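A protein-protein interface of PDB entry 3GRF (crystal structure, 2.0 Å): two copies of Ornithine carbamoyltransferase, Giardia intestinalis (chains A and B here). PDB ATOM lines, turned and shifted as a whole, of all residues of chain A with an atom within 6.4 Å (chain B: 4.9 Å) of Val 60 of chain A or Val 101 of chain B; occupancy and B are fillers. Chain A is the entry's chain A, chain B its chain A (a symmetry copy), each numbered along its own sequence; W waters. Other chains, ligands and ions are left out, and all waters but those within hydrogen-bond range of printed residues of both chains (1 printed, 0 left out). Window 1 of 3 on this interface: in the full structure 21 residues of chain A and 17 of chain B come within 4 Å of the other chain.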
ATOM      1  N   PHE A  51     -29.132  13.819  31.486  1.00  0.00           N
ATOM      2  CA  PHE A  51     -28.630  13.603  32.806  1.00  0.00           C
ATOM      3  C   PHE A  51     -28.949  14.849  33.588  1.00  0.00           C
ATOM      4  O   PHE A  51     -28.543  15.933  33.193  1.00  0.00           O
ATOM      5  CB  PHE A  51     -27.118  13.372  32.766  1.00  0.00           C
ATOM      6  CG  PHE A  51     -26.723  12.020  32.228  1.00  0.00           C
ATOM      7  CD1 PHE A  51     -26.483  10.961  33.084  1.00  0.00           C
ATOM      8  CD2 PHE A  51     -26.573  11.825  30.867  1.00  0.00           C
ATOM      9  CE1 PHE A  51     -26.134   9.714  32.573  1.00  0.00           C
ATOM     10  CE2 PHE A  51     -26.175  10.584  30.336  1.00  0.00           C
ATOM     11  CZ  PHE A  51     -26.003   9.525  31.191  1.00  0.00           C
ATOM     12  N   SER A  55     -23.189  10.894  36.189  1.00  0.00           N
ATOM     13  CA  SER A  55     -22.729   9.632  36.716  1.00  0.00           C
ATOM     14  C   SER A  55     -21.745   9.197  35.679  1.00  0.00           C
ATOM     15  O   SER A  55     -22.127   8.902  34.541  1.00  0.00           O
ATOM     16  CB  SER A  55     -23.851   8.586  36.801  1.00  0.00           C
ATOM     17  OG  SER A  55     -23.329   7.249  36.930  1.00  0.00           O
ATOM     18  N   LEU A  56     -20.486   9.162  36.082  1.00  0.00           N
ATOM     19  CA  LEU A  56     -19.413   8.749  35.224  1.00  0.00           C
ATOM     20  C   LEU A  56     -19.749   7.396  34.656  1.00  0.00           C
ATOM     21  O   LEU A  56     -19.695   7.214  33.457  1.00  0.00           O
ATOM     22  CB  LEU A  56     -18.105   8.667  36.021  1.00  0.00           C
ATOM     23  CG  LEU A  56     -16.897   8.296  35.153  1.00  0.00           C
ATOM     24  CD1 LEU A  56     -15.866   9.399  35.179  1.00  0.00           C
ATOM     25  CD2 LEU A  56     -16.336   6.984  35.615  1.00  0.00           C
ATOM     26  N   ARG A  57     -20.086   6.448  35.534  1.00  0.00           N
ATOM     27  CA  ARG A  57     -20.453   5.080  35.149  1.00  0.00           C
ATOM     28  C   ARG A  57     -21.533   5.053  34.092  1.00  0.00           C
ATOM     29  O   ARG A  57     -21.406   4.366  33.085  1.00  0.00           O
ATOM     30  CB  ARG A  57     -20.968   4.279  36.348  1.00  0.00           C
ATOM     31  CG  ARG A  57     -19.935   3.414  37.028  1.00  0.00           C
ATOM     32  CD  ARG A  57     -20.366   3.279  38.486  1.00  0.00           C
ATOM     33  NE  ARG A  57     -19.435   3.966  39.354  1.00  0.00           N
ATOM     34  CZ  ARG A  57     -19.368   5.287  39.534  1.00  0.00           C
ATOM     35  NH1 ARG A  57     -20.180   6.124  38.898  1.00  0.00           N
ATOM     36  NH2 ARG A  57     -18.451   5.779  40.353  1.00  0.00           N
ATOM     37  N   THR A  58     -22.617   5.791  34.345  1.00  0.00           N
ATOM     38  CA  THR A  58     -23.773   5.717  33.454  1.00  0.00           C
ATOM     39  C   THR A  58     -23.409   6.394  32.135  1.00  0.00           C
ATOM     40  O   THR A  58     -23.604   5.821  31.075  1.00  0.00           O
ATOM     41  CB  THR A  58     -25.072   6.251  34.117  1.00  0.00           C
ATOM     42  OG1 THR A  58     -25.370   5.430  35.255  1.00  0.00           O
ATOM     43  CG2 THR A  58     -26.266   6.206  33.163  1.00  0.00           C
ATOM     44  N   ARG A  59     -22.831   7.583  32.205  1.00  0.00           N
ATOM     45  CA  ARG A  59     -22.508   8.317  31.009  1.00  0.00           C
ATOM     46  C   ARG A  59     -21.477   7.620  30.131  1.00  0.00           C
ATOM     47  O   ARG A  59     -21.640   7.550  28.908  1.00  0.00           O
ATOM     48  CB  ARG A  59     -21.992   9.704  31.344  1.00  0.00           C
ATOM     49  CG  ARG A  59     -22.404  10.702  30.299  1.00  0.00           C
ATOM     50  CD  ARG A  59     -21.240  11.139  29.463  1.00  0.00           C
ATOM     51  NE  ARG A  59     -20.730  12.366  30.018  1.00  0.00           N
ATOM     52  CZ  ARG A  59     -20.212  13.367  29.318  1.00  0.00           C
ATOM     53  NH1 ARG A  59     -20.130  13.326  27.992  1.00  0.00           N
ATOM     54  NH2 ARG A  59     -19.777  14.422  29.985  1.00  0.00           N
ATOM     55  N   VAL A  60     -20.409   7.116  30.731  1.00  0.00           N
ATOM     56  CA  VAL A  60     -19.332   6.533  29.906  1.00  0.00           C
ATOM     57  C   VAL A  60     -19.821   5.235  29.292  1.00  0.00           C
ATOM     58  O   VAL A  60     -19.445   4.894  28.163  1.00  0.00           O
ATOM     59  CB  VAL A  60     -18.012   6.304  30.737  1.00  0.00           C
ATOM     60  CG1 VAL A  60     -17.083   5.253  30.111  1.00  0.00           C
ATOM     61  CG2 VAL A  60     -17.260   7.599  30.941  1.00  0.00           C
ATOM     62  N   SER A  61     -20.612   4.463  30.036  1.00  0.00           N
ATOM     63  CA  SER A  61     -21.023   3.138  29.513  1.00  0.00           C
ATOM     64  C   SER A  61     -22.005   3.304  28.346  1.00  0.00           C
ATOM     65  O   SER A  61     -21.974   2.549  27.372  1.00  0.00           O
ATOM     66  CB  SER A  61     -21.629   2.236  30.618  1.00  0.00           C
ATOM     67  OG  SER A  61     -22.774   2.818  31.200  1.00  0.00           O
ATOM     68  N   LEU A  62     -22.877   4.299  28.476  1.00  0.00           N
ATOM     69  CA  LEU A  62     -23.900   4.649  27.478  1.00  0.00           C
ATOM     70  C   LEU A  62     -23.284   5.164  26.183  1.00  0.00           C
ATOM     71  O   LEU A  62     -23.630   4.692  25.097  1.00  0.00           O
ATOM     72  CB  LEU A  62     -24.824   5.743  28.082  1.00  0.00           C
ATOM     73  CG  LEU A  62     -26.246   5.344  28.481  1.00  0.00           C
ATOM     74  CD1 LEU A  62     -26.441   3.846  28.631  1.00  0.00           C
ATOM     75  CD2 LEU A  62     -26.827   6.119  29.647  1.00  0.00           C
ATOM     76  N   GLU A  63     -22.358   6.129  26.312  1.00  0.00           N
ATOM     77  CA  GLU A  63     -21.726   6.792  25.192  1.00  0.00           C
ATOM     78  C   GLU A  63     -20.799   5.772  24.464  1.00  0.00           C
ATOM     79  O   GLU A  63     -20.783   5.686  23.237  1.00  0.00           O
ATOM     80  CB  GLU A  63     -20.953   8.046  25.694  1.00  0.00           C
ATOM     81  CG  GLU A  63     -21.282   9.327  24.895  1.00  0.00           C
ATOM     82  CD  GLU A  63     -20.791  10.629  25.500  1.00  0.00           C
ATOM     83  OE1 GLU A  63     -21.059  10.905  26.712  1.00  0.00           O
ATOM     84  OE2 GLU A  63     -20.181  11.414  24.747  1.00  0.00           O
ATOM     85  N   THR A  64     -20.060   4.981  25.245  1.00  0.00           N
ATOM     86  CA  THR A  64     -19.195   3.929  24.720  1.00  0.00           C
ATOM     87  C   THR A  64     -19.998   2.807  24.070  1.00  0.00           C
ATOM     88  O   THR A  64     -19.577   2.267  23.017  1.00  0.00           O
ATOM     89  CB  THR A  64     -18.277   3.371  25.845  1.00  0.00           C
ATOM     90  OG1 THR A  64     -17.573   4.448  26.407  1.00  0.00           O
ATOM     91  CG2 THR A  64     -17.199   2.385  25.265  1.00  0.00           C
ATOM     92  N   ALA A  65     -21.144   2.452  24.680  1.00  0.00           N
ATOM     93  CA  ALA A  65     -21.987   1.363  24.162  1.00  0.00           C
ATOM     94  C   ALA A  65     -22.388   1.704  22.762  1.00  0.00           C
ATOM     95  O   ALA A  65     -22.268   0.861  21.872  1.00  0.00           O
ATOM     96  CB  ALA A  65     -23.216   1.104  25.044  1.00  0.00           C
ATOM     97  N   LEU A 311     -21.005  -1.420  30.607  1.00  0.00           N
ATOM     98  CA  LEU A 311     -20.799  -1.208  29.173  1.00  0.00           C
ATOM     99  C   LEU A 311     -21.558  -2.256  28.372  1.00  0.00           C
ATOM    100  O   LEU A 311     -22.404  -1.941  27.554  1.00  0.00           O
ATOM    101  CB  LEU A 311     -19.283  -1.179  28.803  1.00  0.00           C
ATOM    102  CG  LEU A 311     -18.962  -1.299  27.275  1.00  0.00           C
ATOM    103  CD1 LEU A 311     -19.600  -0.173  26.428  1.00  0.00           C
ATOM    104  CD2 LEU A 311     -17.522  -1.485  26.941  1.00  0.00           C
ATOM    105  N   THR B  46     -13.325   4.209  21.639  1.00  0.00           N
ATOM    106  CA  THR B  46     -13.605   5.556  22.195  1.00  0.00           C
ATOM    107  C   THR B  46     -12.492   6.073  23.068  1.00  0.00           C
ATOM    108  O   THR B  46     -11.781   5.315  23.731  1.00  0.00           O
ATOM    109  CB  THR B  46     -14.967   5.646  22.965  1.00  0.00           C
ATOM    110  OG1 THR B  46     -14.703   5.759  24.376  1.00  0.00           O
ATOM    111  CG2 THR B  46     -15.799   4.411  22.677  1.00  0.00           C
ATOM    112  N   LEU B  48     -11.791   8.701  26.193  1.00  0.00           N
ATOM    113  CA  LEU B  48     -12.442   9.410  27.230  1.00  0.00           C
ATOM    114  C   LEU B  48     -11.607  10.639  27.492  1.00  0.00           C
ATOM    115  O   LEU B  48     -10.454  10.524  27.848  1.00  0.00           O
ATOM    116  CB  LEU B  48     -12.449   8.552  28.472  1.00  0.00           C
ATOM    117  CG  LEU B  48     -13.066   9.187  29.710  1.00  0.00           C
ATOM    118  CD1 LEU B  48     -14.406   9.955  29.420  1.00  0.00           C
ATOM    119  CD2 LEU B  48     -13.277   8.078  30.691  1.00  0.00           C
ATOM    120  N   ILE B  74     -15.410  11.073  24.107  1.00  0.00           N
ATOM    121  CA  ILE B  74     -16.333  11.545  25.115  1.00  0.00           C
ATOM    122  C   ILE B  74     -15.721  12.797  25.749  1.00  0.00           C
ATOM    123  O   ILE B  74     -14.668  12.750  26.373  1.00  0.00           O
ATOM    124  CB  ILE B  74     -16.521  10.517  26.206  1.00  0.00           C
ATOM    125  CG1 ILE B  74     -17.186   9.259  25.631  1.00  0.00           C
ATOM    126  CG2 ILE B  74     -17.390  11.094  27.323  1.00  0.00           C
ATOM    127  CD1 ILE B  74     -17.298   8.081  26.650  1.00  0.00           C
ATOM    128  N   TYR B  76     -15.498  14.822  28.640  1.00  0.00           N
ATOM    129  CA  TYR B  76     -15.955  14.765  30.042  1.00  0.00           C
ATOM    130  C   TYR B  76     -15.480  15.959  30.874  1.00  0.00           C
ATOM    131  O   TYR B  76     -14.358  15.992  31.365  1.00  0.00           O
ATOM    132  CB  TYR B  76     -15.556  13.438  30.668  1.00  0.00           C
ATOM    133  CG  TYR B  76     -16.433  13.040  31.823  1.00  0.00           C
ATOM    134  CD1 TYR B  76     -17.267  11.921  31.806  1.00  0.00           C
ATOM    135  CD2 TYR B  76     -16.407  13.827  32.984  1.00  0.00           C
ATOM    136  CE1 TYR B  76     -18.061  11.602  32.916  1.00  0.00           C
ATOM    137  CE2 TYR B  76     -17.197  13.526  34.091  1.00  0.00           C
ATOM    138  CZ  TYR B  76     -18.022  12.420  34.053  1.00  0.00           C
ATOM    139  OH  TYR B  76     -18.796  12.121  35.152  1.00  0.00           O
ATOM    140  N   PHE B  97     -13.003   3.156  34.245  1.00  0.00           N
ATOM    141  CA  PHE B  97     -12.997   3.569  32.824  1.00  0.00           C
ATOM    142  C   PHE B  97     -12.100   2.710  31.939  1.00  0.00           C
ATOM    143  O   PHE B  97     -12.359   2.587  30.758  1.00  0.00           O
ATOM    144  CB  PHE B  97     -12.885   5.106  32.553  1.00  0.00           C
ATOM    145  CG  PHE B  97     -11.567   5.789  32.988  1.00  0.00           C
ATOM    146  CD1 PHE B  97     -11.601   6.814  33.960  1.00  0.00           C
ATOM    147  CD2 PHE B  97     -10.344   5.486  32.389  1.00  0.00           C
ATOM    148  CE1 PHE B  97     -10.427   7.503  34.332  1.00  0.00           C
ATOM    149  CE2 PHE B  97      -9.160   6.154  32.752  1.00  0.00           C
ATOM    150  CZ  PHE B  97      -9.200   7.163  33.718  1.00  0.00           C
ATOM    151  N   SER B  98     -11.091   2.078  32.551  1.00  0.00           N
ATOM    152  CA  SER B  98     -10.145   1.203  31.866  1.00  0.00           C
ATOM    153  C   SER B  98     -10.762  -0.127  31.468  1.00  0.00           C
ATOM    154  O   SER B  98     -10.162  -0.874  30.718  1.00  0.00           O
ATOM    155  CB  SER B  98      -8.918   0.917  32.719  1.00  0.00           C
ATOM    156  OG  SER B  98      -8.389   2.092  33.279  1.00  0.00           O
ATOM    157  N   ARG B  99     -11.953  -0.417  31.949  1.00  0.00           N
ATOM    158  CA  ARG B  99     -12.669  -1.608  31.497  1.00  0.00           C
ATOM    159  C   ARG B  99     -13.811  -1.237  30.552  1.00  0.00           C
ATOM    160  O   ARG B  99     -14.675  -2.070  30.288  1.00  0.00           O
ATOM    161  CB  ARG B  99     -13.237  -2.303  32.711  1.00  0.00           C
ATOM    162  CG  ARG B  99     -12.226  -2.980  33.578  1.00  0.00           C
ATOM    163  CD  ARG B  99     -12.920  -3.326  34.885  1.00  0.00           C
ATOM    164  NE  ARG B  99     -12.156  -4.221  35.776  1.00  0.00           N
ATOM    165  CZ  ARG B  99     -11.060  -3.859  36.443  1.00  0.00           C
ATOM    166  NH1 ARG B  99     -10.570  -2.629  36.331  1.00  0.00           N
ATOM    167  NH2 ARG B  99     -10.468  -4.720  37.240  1.00  0.00           N
ATOM    168  N   MET B 100     -13.865   0.037  30.120  1.00  0.00           N
ATOM    169  CA  MET B 100     -14.908   0.521  29.176  1.00  0.00           C
ATOM    170  C   MET B 100     -14.307   1.174  27.939  1.00  0.00           C
ATOM    171  O   MET B 100     -14.607   0.742  26.819  1.00  0.00           O
ATOM    172  CB  MET B 100     -15.922   1.473  29.838  1.00  0.00           C
ATOM    173  CG  MET B 100     -16.948   0.793  30.801  1.00  0.00           C
ATOM    174  SD  MET B 100     -18.040   2.018  31.544  1.00  0.00           S
ATOM    175  CE  MET B 100     -18.664   1.161  32.958  1.00  0.00           C
ATOM    176  N   VAL B 101     -13.446   2.195  28.156  1.00  0.00           N
ATOM    177  CA  VAL B 101     -12.844   2.970  27.070  1.00  0.00           C
ATOM    178  C   VAL B 101     -11.502   2.352  26.649  1.00  0.00           C
ATOM    179  O   VAL B 101     -10.968   1.455  27.326  1.00  0.00           O
ATOM    180  CB  VAL B 101     -12.753   4.472  27.424  1.00  0.00           C
ATOM    181  CG1 VAL B 101     -14.157   4.971  27.798  1.00  0.00           C
ATOM    182  CG2 VAL B 101     -11.747   4.701  28.596  1.00  0.00           C
ATOM    183  N   ASP B 102     -11.019   2.767  25.479  1.00  0.00           N
ATOM    184  CA  ASP B 102      -9.785   2.259  24.902  1.00  0.00           C
ATOM    185  C   ASP B 102      -8.599   3.168  25.206  1.00  0.00           C
ATOM    186  O   ASP B 102      -7.425   2.761  25.171  1.00  0.00           O
ATOM    187  CB  ASP B 102      -9.972   2.102  23.403  1.00  0.00           C
ATOM    188  CG  ASP B 102     -11.083   1.190  23.078  1.00  0.00           C
ATOM    189  OD1 ASP B 102     -12.190   1.675  22.764  1.00  0.00           O
ATOM    190  OD2 ASP B 102     -10.882  -0.023  23.216  1.00  0.00           O
ATOM    191  N   ILE B 103      -8.891   4.428  25.488  1.00  0.00           N
ATOM    192  CA  ILE B 103      -7.820   5.399  25.686  1.00  0.00           C
ATOM    193  C   ILE B 103      -8.379   6.593  26.396  1.00  0.00           C
ATOM    194  O   ILE B 103      -9.586   6.787  26.373  1.00  0.00           O
ATOM    195  CB  ILE B 103      -7.144   5.844  24.343  1.00  0.00           C
ATOM    196  CG1 ILE B 103      -5.984   6.795  24.594  1.00  0.00           C
ATOM    197  CG2 ILE B 103      -8.121   6.453  23.331  1.00  0.00           C
ATOM    198  CD1 ILE B 103      -5.038   6.837  23.466  1.00  0.00           C
ATOM    199  N   VAL B 123      -5.639   1.554  30.674  1.00  0.00           N
ATOM    200  CA  VAL B 123      -5.620   1.943  29.250  1.00  0.00           C
ATOM    201  C   VAL B 123      -4.615   3.092  29.160  1.00  0.00           C
ATOM    202  O   VAL B 123      -4.327   3.721  30.157  1.00  0.00           O
ATOM    203  CB  VAL B 123      -7.044   2.387  28.732  1.00  0.00           C
ATOM    204  CG1 VAL B 123      -8.028   1.223  28.744  1.00  0.00           C
ATOM    205  CG2 VAL B 123      -7.607   3.528  29.569  1.00  0.00           C
HETATM  206  O   HOH W   1     -21.356  11.754  33.654  1.00  0.00           O
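Water W1 bridges the side-chain hydroxyl (OH) of Tyr 76 of chain B (3.0 Å) and the backbone carbonyl oxygen (O) of Ser 55 of chain A (3.1 Å).
O of Arg 57 of chain A lies within hydrogen-bond range of OG of Ser 61 of chain A. O of Thr 58 of chain A is in hydrogen-bond range of OG of Ser 61 of chain A (3.1 Å). NH1 of Arg 59 of chain A is in salt-bridge range of OE1 of Glu 63 of chain A, 2.9 Å away. The side-chain hydroxyl (OG1) of Thr 64 of chain A is in hydrogen-bond range of the backbone carbonyl oxygen (O) of Val 60 of chain A (2.6 Å). The side-chain carboxylate (OD1) of Asp 102 of chain B is in hydrogen-bond range of the backbone NH (N) of Thr 46 of chain B (3.0 Å). O of Thr 46 of chain B is in hydrogen-bond range of N of Ile 103 of chain B.
Printed residues of chain B that touch a printed residue of chain A: Thr 46, Ile 74, Tyr 76, Met 100 and Val 101. Along chain A the printed residues that touch a printed residue of chain B span positions 56 to 311. Among the printed residues, no Asp or Glu carboxylate lies within 4 Å of a Lys or Arg side-chain nitrogen of the other chain.
No position is printed for both chains. Of the 12 pairs that touch across the chains among the printed residues, none has its exchanged pair printed and touching as well.
Among the printed residues, pairs that only touch across the chains: Leu 56 of chain A with Tyr 76 of chain B, Arg 59 of chain A with Ile 74 of chain B, Arg 59 of chain A with Tyr 76 of chain B, Val 60 of chain A with Met 100 of chain B, Val 60 of chain A with Val 101 of chain B, Ser 61 of chain A with Met 100 of chain B, Glu 63 of chain A with Ile 74 of chain B, Thr 64 of chain A with Thr 46 of chain B, Thr 64 of chain A with Ile 74 of chain B, Thr 64 of chain A with Met 100 of chain B, Thr 64 of chain A with Val 101 of chain B and Leu 311 of chain A with Met 100 of chain B.
Of the printed residues of chain B, Val 60 of chain A touches Met 100 (3.7 Å) and Val 101 (3.7 Å). Val 101 of chain B touches just these residues of chain A: Val 60 and Thr 64. Printed residues of chain B within 4 Å of Ser 61 of chain A: Met 100 (3.7 Å). Of the printed residues of chain B, Leu 56 of chain A touches Tyr 76 (3.4 Å). Leu 62 of chain A touches none of the printed residues of chain B. Ala 65 of chain A touches none of the printed residues of chain B. The nearest printed residue of chain B that does not touch Val 60 of chain A is Leu 48 of chain B (4.001 Å). The nearest printed residue of chain A that does not touch Thr 46 of chain B is Glu 63 of chain A (5.2 Å).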
